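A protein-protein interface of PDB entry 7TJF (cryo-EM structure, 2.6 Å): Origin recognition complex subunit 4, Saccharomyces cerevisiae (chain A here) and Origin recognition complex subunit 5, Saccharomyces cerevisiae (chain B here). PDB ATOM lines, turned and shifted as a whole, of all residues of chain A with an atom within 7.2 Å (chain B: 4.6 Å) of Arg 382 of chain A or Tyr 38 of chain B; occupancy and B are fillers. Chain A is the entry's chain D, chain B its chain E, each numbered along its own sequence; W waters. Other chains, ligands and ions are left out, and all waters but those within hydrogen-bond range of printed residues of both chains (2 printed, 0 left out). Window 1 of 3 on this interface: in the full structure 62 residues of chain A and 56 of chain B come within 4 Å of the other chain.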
ATOM      1  N   LEU A 375     -34.096  17.921   0.649  1.00  0.00           N
ATOM      2  CA  LEU A 375     -32.920  17.898   1.507  1.00  0.00           C
ATOM      3  C   LEU A 375     -31.979  16.738   1.199  1.00  0.00           C
ATOM      4  O   LEU A 375     -31.045  16.499   1.966  1.00  0.00           O
ATOM      5  CB  LEU A 375     -33.339  17.837   2.976  1.00  0.00           C
ATOM      6  CG  LEU A 375     -34.293  18.910   3.490  1.00  0.00           C
ATOM      7  CD1 LEU A 375     -35.018  18.416   4.728  1.00  0.00           C
ATOM      8  CD2 LEU A 375     -33.543  20.197   3.775  1.00  0.00           C
ATOM      9  N   SER A 376     -32.202  16.010   0.105  1.00  0.00           N
ATOM     10  CA  SER A 376     -31.461  14.774  -0.127  1.00  0.00           C
ATOM     11  C   SER A 376     -30.020  15.004  -0.580  1.00  0.00           C
ATOM     12  O   SER A 376     -29.207  14.079  -0.485  1.00  0.00           O
ATOM     13  CB  SER A 376     -32.206  13.905  -1.144  1.00  0.00           C
ATOM     14  OG  SER A 376     -32.107  14.436  -2.451  1.00  0.00           O
ATOM     15  N   ASN A 377     -29.680  16.203  -1.060  1.00  0.00           N
ATOM     16  CA  ASN A 377     -28.324  16.500  -1.516  1.00  0.00           C
ATOM     17  C   ASN A 377     -27.624  17.558  -0.670  1.00  0.00           C
ATOM     18  O   ASN A 377     -26.668  18.178  -1.144  1.00  0.00           O
ATOM     19  CB  ASN A 377     -28.310  16.934  -2.985  1.00  0.00           C
ATOM     20  CG  ASN A 377     -28.679  15.816  -3.929  1.00  0.00           C
ATOM     21  OD1 ASN A 377     -28.244  14.680  -3.759  1.00  0.00           O
ATOM     22  ND2 ASN A 377     -29.459  16.137  -4.950  1.00  0.00           N
ATOM     23  N   ASN A 378     -28.062  17.788   0.564  1.00  0.00           N
ATOM     24  CA  ASN A 378     -27.312  18.663   1.454  1.00  0.00           C
ATOM     25  C   ASN A 378     -26.201  17.853   2.132  1.00  0.00           C
ATOM     26  O   ASN A 378     -25.947  16.700   1.777  1.00  0.00           O
ATOM     27  CB  ASN A 378     -28.258  19.395   2.420  1.00  0.00           C
ATOM     28  CG  ASN A 378     -29.051  18.468   3.355  1.00  0.00           C
ATOM     29  OD1 ASN A 378     -28.761  17.284   3.526  1.00  0.00           O
ATOM     30  ND2 ASN A 378     -30.085  19.034   3.965  1.00  0.00           N
ATOM     31  N   LEU A 379     -25.539  18.441   3.131  1.00  0.00           N
ATOM     32  CA  LEU A 379     -24.415  17.771   3.781  1.00  0.00           C
ATOM     33  C   LEU A 379     -24.826  16.558   4.609  1.00  0.00           C
ATOM     34  O   LEU A 379     -23.960  15.747   4.947  1.00  0.00           O
ATOM     35  CB  LEU A 379     -23.653  18.757   4.669  1.00  0.00           C
ATOM     36  CG  LEU A 379     -22.406  19.419   4.076  1.00  0.00           C
ATOM     37  CD1 LEU A 379     -21.646  20.157   5.158  1.00  0.00           C
ATOM     38  CD2 LEU A 379     -21.504  18.407   3.388  1.00  0.00           C
ATOM     39  N   THR A 380     -26.111  16.399   4.922  1.00  0.00           N
ATOM     40  CA  THR A 380     -26.579  15.227   5.649  1.00  0.00           C
ATOM     41  C   THR A 380     -26.795  14.035   4.723  1.00  0.00           C
ATOM     42  O   THR A 380     -26.237  12.961   4.957  1.00  0.00           O
ATOM     43  CB  THR A 380     -27.873  15.550   6.400  1.00  0.00           C
ATOM     44  OG1 THR A 380     -27.626  16.585   7.358  1.00  0.00           O
ATOM     45  CG2 THR A 380     -28.395  14.320   7.122  1.00  0.00           C
ATOM     46  N   GLY A 381     -27.591  14.213   3.663  1.00  0.00           N
ATOM     47  CA  GLY A 381     -27.843  13.134   2.723  1.00  0.00           C
ATOM     48  C   GLY A 381     -26.640  12.737   1.896  1.00  0.00           C
ATOM     49  O   GLY A 381     -26.570  11.595   1.430  1.00  0.00           O
ATOM     50  N   ARG A 382     -25.691  13.654   1.704  1.00  0.00           N
ATOM     51  CA  ARG A 382     -24.447  13.311   1.025  1.00  0.00           C
ATOM     52  C   ARG A 382     -23.551  12.461   1.917  1.00  0.00           C
ATOM     53  O   ARG A 382     -22.774  11.637   1.421  1.00  0.00           O
ATOM     54  CB  ARG A 382     -23.730  14.588   0.596  1.00  0.00           C
ATOM     55  CG  ARG A 382     -23.895  14.933  -0.866  1.00  0.00           C
ATOM     56  CD  ARG A 382     -23.054  16.138  -1.216  1.00  0.00           C
ATOM     57  NE  ARG A 382     -23.679  17.351  -0.704  1.00  0.00           N
ATOM     58  CZ  ARG A 382     -23.023  18.440  -0.332  1.00  0.00           C
ATOM     59  NH1 ARG A 382     -21.705  18.512  -0.409  1.00  0.00           N
ATOM     60  NH2 ARG A 382     -23.707  19.479   0.133  1.00  0.00           N
ATOM     61  N   LEU A 383     -23.636  12.665   3.236  1.00  0.00           N
ATOM     62  CA  LEU A 383     -22.860  11.870   4.183  1.00  0.00           C
ATOM     63  C   LEU A 383     -23.287  10.407   4.180  1.00  0.00           C
ATOM     64  O   LEU A 383     -22.440   9.511   4.266  1.00  0.00           O
ATOM     65  CB  LEU A 383     -22.986  12.459   5.586  1.00  0.00           C
ATOM     66  CG  LEU A 383     -21.997  11.923   6.618  1.00  0.00           C
ATOM     67  CD1 LEU A 383     -20.587  12.163   6.146  1.00  0.00           C
ATOM     68  CD2 LEU A 383     -22.226  12.579   7.963  1.00  0.00           C
ATOM     69  N   GLN A 384     -24.591  10.143   4.072  1.00  0.00           N
ATOM     70  CA  GLN A 384     -25.083   8.770   4.088  1.00  0.00           C
ATOM     71  C   GLN A 384     -24.805   8.011   2.794  1.00  0.00           C
ATOM     72  O   GLN A 384     -24.995   6.791   2.767  1.00  0.00           O
ATOM     73  CB  GLN A 384     -26.585   8.753   4.383  1.00  0.00           C
ATOM     74  CG  GLN A 384     -27.031   9.816   5.368  1.00  0.00           C
ATOM     75  CD  GLN A 384     -28.239   9.402   6.186  1.00  0.00           C
ATOM     76  OE1 GLN A 384     -29.139   8.725   5.692  1.00  0.00           O
ATOM     77  NE2 GLN A 384     -28.264   9.811   7.450  1.00  0.00           N
ATOM     78  N   SER A 385     -24.365   8.685   1.733  1.00  0.00           N
ATOM     79  CA  SER A 385     -24.041   8.024   0.476  1.00  0.00           C
ATOM     80  C   SER A 385     -22.581   7.594   0.385  1.00  0.00           C
ATOM     81  O   SER A 385     -22.197   6.965  -0.606  1.00  0.00           O
ATOM     82  CB  SER A 385     -24.375   8.940  -0.706  1.00  0.00           C
ATOM     83  OG  SER A 385     -23.387   9.942  -0.873  1.00  0.00           O
ATOM     84  N   LEU A 386     -21.766   7.910   1.386  1.00  0.00           N
ATOM     85  CA  LEU A 386     -20.342   7.623   1.329  1.00  0.00           C
ATOM     86  C   LEU A 386     -20.059   6.155   1.629  1.00  0.00           C
ATOM     87  O   LEU A 386     -20.827   5.479   2.319  1.00  0.00           O
ATOM     88  CB  LEU A 386     -19.584   8.507   2.320  1.00  0.00           C
ATOM     89  CG  LEU A 386     -19.507   9.999   1.995  1.00  0.00           C
ATOM     90  CD1 LEU A 386     -18.631  10.723   3.006  1.00  0.00           C
ATOM     91  CD2 LEU A 386     -18.996  10.226   0.576  1.00  0.00           C
ATOM     92  N   SER A 387     -18.944   5.666   1.093  1.00  0.00           N
ATOM     93  CA  SER A 387     -18.437   4.349   1.444  1.00  0.00           C
ATOM     94  C   SER A 387     -17.638   4.427   2.744  1.00  0.00           C
ATOM     95  O   SER A 387     -17.353   5.508   3.263  1.00  0.00           O
ATOM     96  CB  SER A 387     -17.581   3.778   0.314  1.00  0.00           C
ATOM     97  OG  SER A 387     -16.313   4.408   0.249  1.00  0.00           O
ATOM     98  N   LEU A 466     -13.983  13.093  -2.644  1.00  0.00           N
ATOM     99  CA  LEU A 466     -14.407  13.920  -1.519  1.00  0.00           C
ATOM    100  C   LEU A 466     -14.273  15.405  -1.831  1.00  0.00           C
ATOM    101  O   LEU A 466     -15.055  16.215  -1.321  1.00  0.00           O
ATOM    102  CB  LEU A 466     -13.601  13.572  -0.270  1.00  0.00           C
ATOM    103  CG  LEU A 466     -13.949  12.259   0.434  1.00  0.00           C
ATOM    104  CD1 LEU A 466     -12.921  11.941   1.504  1.00  0.00           C
ATOM    105  CD2 LEU A 466     -15.353  12.307   1.022  1.00  0.00           C
ATOM    106  N   GLN A 468     -14.659  16.554  -4.938  1.00  0.00           N
ATOM    107  CA  GLN A 468     -15.710  16.778  -5.927  1.00  0.00           C
ATOM    108  C   GLN A 468     -17.092  16.886  -5.286  1.00  0.00           C
ATOM    109  O   GLN A 468     -17.925  17.674  -5.745  1.00  0.00           O
ATOM    110  CB  GLN A 468     -15.683  15.656  -6.968  1.00  0.00           C
ATOM    111  CG  GLN A 468     -16.672  15.808  -8.112  1.00  0.00           C
ATOM    112  CD  GLN A 468     -16.144  15.246  -9.419  1.00  0.00           C
ATOM    113  OE1 GLN A 468     -16.594  14.200  -9.886  1.00  0.00           O
ATOM    114  NE2 GLN A 468     -15.185  15.942 -10.018  1.00  0.00           N
ATOM    115  N   LEU A 469     -17.342  16.142  -4.209  1.00  0.00           N
ATOM    116  CA  LEU A 469     -18.619  16.193  -3.504  1.00  0.00           C
ATOM    117  C   LEU A 469     -18.706  17.328  -2.492  1.00  0.00           C
ATOM    118  O   LEU A 469     -19.639  17.323  -1.679  1.00  0.00           O
ATOM    119  CB  LEU A 469     -18.890  14.862  -2.799  1.00  0.00           C
ATOM    120  CG  LEU A 469     -19.477  13.750  -3.664  1.00  0.00           C
ATOM    121  CD1 LEU A 469     -19.320  12.412  -2.975  1.00  0.00           C
ATOM    122  CD2 LEU A 469     -20.935  14.033  -3.980  1.00  0.00           C
ATOM    123  N   ASP A 470     -17.746  18.262  -2.518  1.00  0.00           N
ATOM    124  CA  ASP A 470     -17.721  19.487  -1.708  1.00  0.00           C
ATOM    125  C   ASP A 470     -17.672  19.170  -0.206  1.00  0.00           C
ATOM    126  O   ASP A 470     -18.194  19.908   0.633  1.00  0.00           O
ATOM    127  CB  ASP A 470     -18.898  20.411  -2.074  1.00  0.00           C
ATOM    128  CG  ASP A 470     -18.717  21.843  -1.582  1.00  0.00           C
ATOM    129  OD1 ASP A 470     -17.576  22.353  -1.623  1.00  0.00           O
ATOM    130  OD2 ASP A 470     -19.717  22.454  -1.151  1.00  0.00           O
ATOM    131  N   PHE A 471     -17.048  18.049   0.153  1.00  0.00           N
ATOM    132  CA  PHE A 471     -16.715  17.826   1.554  1.00  0.00           C
ATOM    133  C   PHE A 471     -15.473  18.609   1.962  1.00  0.00           C
ATOM    134  O   PHE A 471     -15.377  19.056   3.109  1.00  0.00           O
ATOM    135  CB  PHE A 471     -16.524  16.333   1.826  1.00  0.00           C
ATOM    136  CG  PHE A 471     -17.807  15.545   1.840  1.00  0.00           C
ATOM    137  CD1 PHE A 471     -18.687  15.648   2.904  1.00  0.00           C
ATOM    138  CD2 PHE A 471     -18.125  14.692   0.792  1.00  0.00           C
ATOM    139  CE1 PHE A 471     -19.868  14.920   2.923  1.00  0.00           C
ATOM    140  CE2 PHE A 471     -19.305  13.960   0.804  1.00  0.00           C
ATOM    141  CZ  PHE A 471     -20.176  14.078   1.873  1.00  0.00           C
ATOM    142  N   GLN A 510     -15.687  21.399   5.183  1.00  0.00           N
ATOM    143  CA  GLN A 510     -17.034  21.947   5.151  1.00  0.00           C
ATOM    144  C   GLN A 510     -17.931  21.352   6.225  1.00  0.00           C
ATOM    145  O   GLN A 510     -19.025  21.874   6.456  1.00  0.00           O
ATOM    146  CB  GLN A 510     -17.675  21.729   3.775  1.00  0.00           C
ATOM    147  CG  GLN A 510     -17.114  22.614   2.677  1.00  0.00           C
ATOM    148  CD  GLN A 510     -17.859  23.929   2.530  1.00  0.00           C
ATOM    149  OE1 GLN A 510     -18.276  24.540   3.513  1.00  0.00           O
ATOM    150  NE2 GLN A 510     -18.022  24.372   1.294  1.00  0.00           N
ATOM    151  N   GLN B  36     -31.409  18.821 -10.007  1.00  0.00           N
ATOM    152  CA  GLN B  36     -30.119  18.919  -9.336  1.00  0.00           C
ATOM    153  C   GLN B  36     -29.664  17.546  -8.864  1.00  0.00           C
ATOM    154  O   GLN B  36     -30.406  16.844  -8.175  1.00  0.00           O
ATOM    155  CB  GLN B  36     -30.182  19.886  -8.153  1.00  0.00           C
ATOM    156  CG  GLN B  36     -28.820  20.239  -7.568  1.00  0.00           C
ATOM    157  CD  GLN B  36     -28.452  19.379  -6.373  1.00  0.00           C
ATOM    158  OE1 GLN B  36     -29.274  19.134  -5.494  1.00  0.00           O
ATOM    159  NE2 GLN B  36     -27.211  18.909  -6.343  1.00  0.00           N
ATOM    160  N   GLY B  37     -28.439  17.184  -9.217  1.00  0.00           N
ATOM    161  CA  GLY B  37     -27.855  15.943  -8.753  1.00  0.00           C
ATOM    162  C   GLY B  37     -26.395  15.887  -9.125  1.00  0.00           C
ATOM    163  O   GLY B  37     -25.942  16.575 -10.044  1.00  0.00           O
ATOM    164  N   TYR B  38     -25.661  15.046  -8.407  1.00  0.00           N
ATOM    165  CA  TYR B  38     -24.240  14.895  -8.675  1.00  0.00           C
ATOM    166  C   TYR B  38     -24.031  13.926  -9.835  1.00  0.00           C
ATOM    167  O   TYR B  38     -24.982  13.474 -10.479  1.00  0.00           O
ATOM    168  CB  TYR B  38     -23.507  14.470  -7.406  1.00  0.00           C
ATOM    169  CG  TYR B  38     -23.421  15.598  -6.407  1.00  0.00           C
ATOM    170  CD1 TYR B  38     -22.386  16.523  -6.464  1.00  0.00           C
ATOM    171  CD2 TYR B  38     -24.401  15.767  -5.437  1.00  0.00           C
ATOM    172  CE1 TYR B  38     -22.315  17.570  -5.564  1.00  0.00           C
ATOM    173  CE2 TYR B  38     -24.341  16.811  -4.537  1.00  0.00           C
ATOM    174  CZ  TYR B  38     -23.296  17.708  -4.603  1.00  0.00           C
ATOM    175  OH  TYR B  38     -23.230  18.746  -3.706  1.00  0.00           O
ATOM    176  N   SER B  39     -22.767  13.624 -10.122  1.00  0.00           N
ATOM    177  CA  SER B  39     -22.417  12.870 -11.320  1.00  0.00           C
ATOM    178  C   SER B  39     -22.885  11.423 -11.229  1.00  0.00           C
ATOM    179  O   SER B  39     -22.748  10.769 -10.192  1.00  0.00           O
ATOM    180  CB  SER B  39     -20.908  12.916 -11.551  1.00  0.00           C
ATOM    181  OG  SER B  39     -20.533  14.116 -12.198  1.00  0.00           O
ATOM    182  N   GLY B  40     -23.449  10.932 -12.329  1.00  0.00           N
ATOM    183  CA  GLY B  40     -23.939   9.572 -12.383  1.00  0.00           C
ATOM    184  C   GLY B  40     -25.190   9.311 -11.583  1.00  0.00           C
ATOM    185  O   GLY B  40     -25.438   8.168 -11.198  1.00  0.00           O
ATOM    186  N   THR B  41     -25.989  10.338 -11.314  1.00  0.00           N
ATOM    187  CA  THR B  41     -27.228  10.169 -10.574  1.00  0.00           C
ATOM    188  C   THR B  41     -28.424   9.938 -11.486  1.00  0.00           C
ATOM    189  O   THR B  41     -29.555   9.860 -11.000  1.00  0.00           O
ATOM    190  CB  THR B  41     -27.478  11.378  -9.666  1.00  0.00           C
ATOM    191  OG1 THR B  41     -27.236  12.590 -10.390  1.00  0.00           O
ATOM    192  CG2 THR B  41     -26.558  11.324  -8.454  1.00  0.00           C
ATOM    193  N   LYS B  43     -29.700  11.892 -14.032  1.00  0.00           N
ATOM    194  CA  LYS B  43     -30.514  13.025 -14.468  1.00  0.00           C
ATOM    195  C   LYS B  43     -30.762  12.981 -15.972  1.00  0.00           C
ATOM    196  O   LYS B  43     -31.912  13.080 -16.428  1.00  0.00           O
ATOM    197  CB  LYS B  43     -29.838  14.343 -14.080  1.00  0.00           C
ATOM    198  CG  LYS B  43     -29.303  14.398 -12.660  1.00  0.00           C
ATOM    199  CD  LYS B  43     -28.479  15.657 -12.427  1.00  0.00           C
ATOM    200  CE  LYS B  43     -27.101  15.571 -13.079  1.00  0.00           C
ATOM    201  NZ  LYS B  43     -26.129  14.753 -12.308  1.00  0.00           N
ATOM    202  N   LEU B 171     -25.083  20.455 -10.996  1.00  0.00           N
ATOM    203  CA  LEU B 171     -24.351  19.478 -10.199  1.00  0.00           C
ATOM    204  C   LEU B 171     -24.260  19.875  -8.729  1.00  0.00           C
ATOM    205  O   LEU B 171     -24.695  19.125  -7.853  1.00  0.00           O
ATOM    206  CB  LEU B 171     -22.943  19.286 -10.783  1.00  0.00           C
ATOM    207  CG  LEU B 171     -22.778  18.366 -11.995  1.00  0.00           C
ATOM    208  CD1 LEU B 171     -21.409  18.550 -12.627  1.00  0.00           C
ATOM    209  CD2 LEU B 171     -22.998  16.916 -11.618  1.00  0.00           C
ATOM    210  N   GLU B 172     -23.695  21.043  -8.446  1.00  0.00           N
ATOM    211  CA  GLU B 172     -23.335  21.400  -7.082  1.00  0.00           C
ATOM    212  C   GLU B 172     -24.531  21.951  -6.316  1.00  0.00           C
ATOM    213  O   GLU B 172     -25.331  22.725  -6.851  1.00  0.00           O
ATOM    214  CB  GLU B 172     -22.196  22.417  -7.081  1.00  0.00           C
ATOM    215  CG  GLU B 172     -20.937  21.922  -7.777  1.00  0.00           C
ATOM    216  CD  GLU B 172     -20.191  23.027  -8.499  1.00  0.00           C
ATOM    217  OE1 GLU B 172     -20.818  24.057  -8.832  1.00  0.00           O
ATOM    218  OE2 GLU B 172     -18.975  22.870  -8.735  1.00  0.00           O
ATOM    219  N   THR B 173     -24.647  21.529  -5.056  1.00  0.00           N
ATOM    220  CA  THR B 173     -25.723  21.995  -4.188  1.00  0.00           C
ATOM    221  C   THR B 173     -25.589  23.482  -3.873  1.00  0.00           C
ATOM    222  O   THR B 173     -26.582  24.212  -3.910  1.00  0.00           O
ATOM    223  CB  THR B 173     -25.744  21.159  -2.905  1.00  0.00           C
ATOM    224  OG1 THR B 173     -25.972  19.785  -3.236  1.00  0.00           O
ATOM    225  CG2 THR B 173     -26.828  21.626  -1.944  1.00  0.00           C
ATOM    226  N   PHE B 189     -31.854  14.511  -7.392  1.00  0.00           N
ATOM    227  CA  PHE B 189     -31.414  13.180  -7.798  1.00  0.00           C
ATOM    228  C   PHE B 189     -30.331  12.776  -6.809  1.00  0.00           C
ATOM    229  O   PHE B 189     -29.144  13.067  -7.020  1.00  0.00           O
ATOM    230  CB  PHE B 189     -30.895  13.178  -9.235  1.00  0.00           C
ATOM    231  CG  PHE B 189     -31.978  13.208 -10.275  1.00  0.00           C
ATOM    232  CD1 PHE B 189     -32.660  14.383 -10.559  1.00  0.00           C
ATOM    233  CD2 PHE B 189     -32.297  12.065 -10.988  1.00  0.00           C
ATOM    234  CE1 PHE B 189     -33.650  14.409 -11.517  1.00  0.00           C
ATOM    235  CE2 PHE B 189     -33.282  12.085 -11.951  1.00  0.00           C
ATOM    236  CZ  PHE B 189     -33.962  13.257 -12.215  1.00  0.00           C
HETATM  237  O   HOH W   1     -21.825  21.768  -3.250  1.00  0.00           O
HETATM  238  O   HOH W   2     -26.793  13.687  -6.078  1.00  0.00           O
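Printed residues of chain B within 4 Å of Leu 469 of chain A: Tyr 38 (3.8 Å). Of the printed residues of chain A, Gln 36 of chain B touches Asn 377 (3.1 Å). Of the printed residues of chain A, Thr 173 of chain B touches Asn 377. The nearest residue of chain B that does not touch Arg 382 of chain A is Thr 173 of chain B (4.03 Å). The nearest printed residue of chain A that does not touch Gln 36 of chain B is Ser 376 of chain A (6.3 Å).
Among the printed residues, merely in contact across the chains: Asn 377 of chain A with Phe 189 of chain B (3.7 Å) and Leu 469 of chain A with Tyr 38 of chain B (3.8 Å).
The side-chain amide oxygen (OE1) of Gln 36 of chain B is in hydrogen-bond range of the side-chain amide nitrogen (ND2) of Asn 377 of chain A, at 3.1 Å. The side-chain hydroxyl (OG1) of Thr 173 of chain B lies within hydrogen-bond range of the backbone carbonyl oxygen (O) of Asn 377 of chain A (2.7 Å). NE of Arg 382 of chain A is in hydrogen-bond range of OH of Tyr 38 of chain B (3.3 Å).
Water W2 lies within hydrogen-bond range of the backbone carbonyl oxygen of Phe 189 of chain B (2.6 Å), the side-chain amide oxygen of Asn 377 of chain A (2.9 Å) and the backbone NH of Tyr 38 of chain B (2.9 Å). Water W1 lies within hydrogen-bond range of the side-chain carboxylate of Asp 470 of chain A (3.1 Å), the backbone NH of Thr 173 of chain B (3.4 Å) and the side-chain hydroxyl of Tyr 38 of chain B (3.4 Å).
Of the 19 printed residues of chain A, 3 touch a printed residue of chain B. Hydrophobic or aromatic side chains of chain B that line the printed part of chain A: Tyr 38. Along chain B the printed residues that touch a printed residue of chain A span positions 36 to 189. Among the printed residues, 5 pairs touch across the chains. Among the printed residues, no Asp or Glu carboxylate lies within 4 Å of a Lys or Arg side-chain nitrogen of the other chain.
The guanidinium group (NE) of Arg 382 of chain A lies close to the backbone carbonyl oxygen (O) of Asn 378 of chain A (3.4 Å). The side-chain hydroxyl (OG) of Ser 385 of chain A lies within hydrogen-bond range of the backbone carbonyl oxygen (O) of Arg 382 of chain A (2.9 Å). NH1 of Arg 382 of chain A lies within hydrogen-bond range of O of Leu 469 of chain A (2.7 Å). OG1 of Thr 173 of chain B sits at hydrogen-bond distance from NE2 of Gln 36 of chain B (3.5 Å). O of Tyr 38 of chain B is in hydrogen-bond range of NZ of Lys 43 of chain B (2.5 Å). OH of Tyr 38 of chain B is in hydrogen-bond range of OG1 of Thr 173 of chain B, 3.0 Å away.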
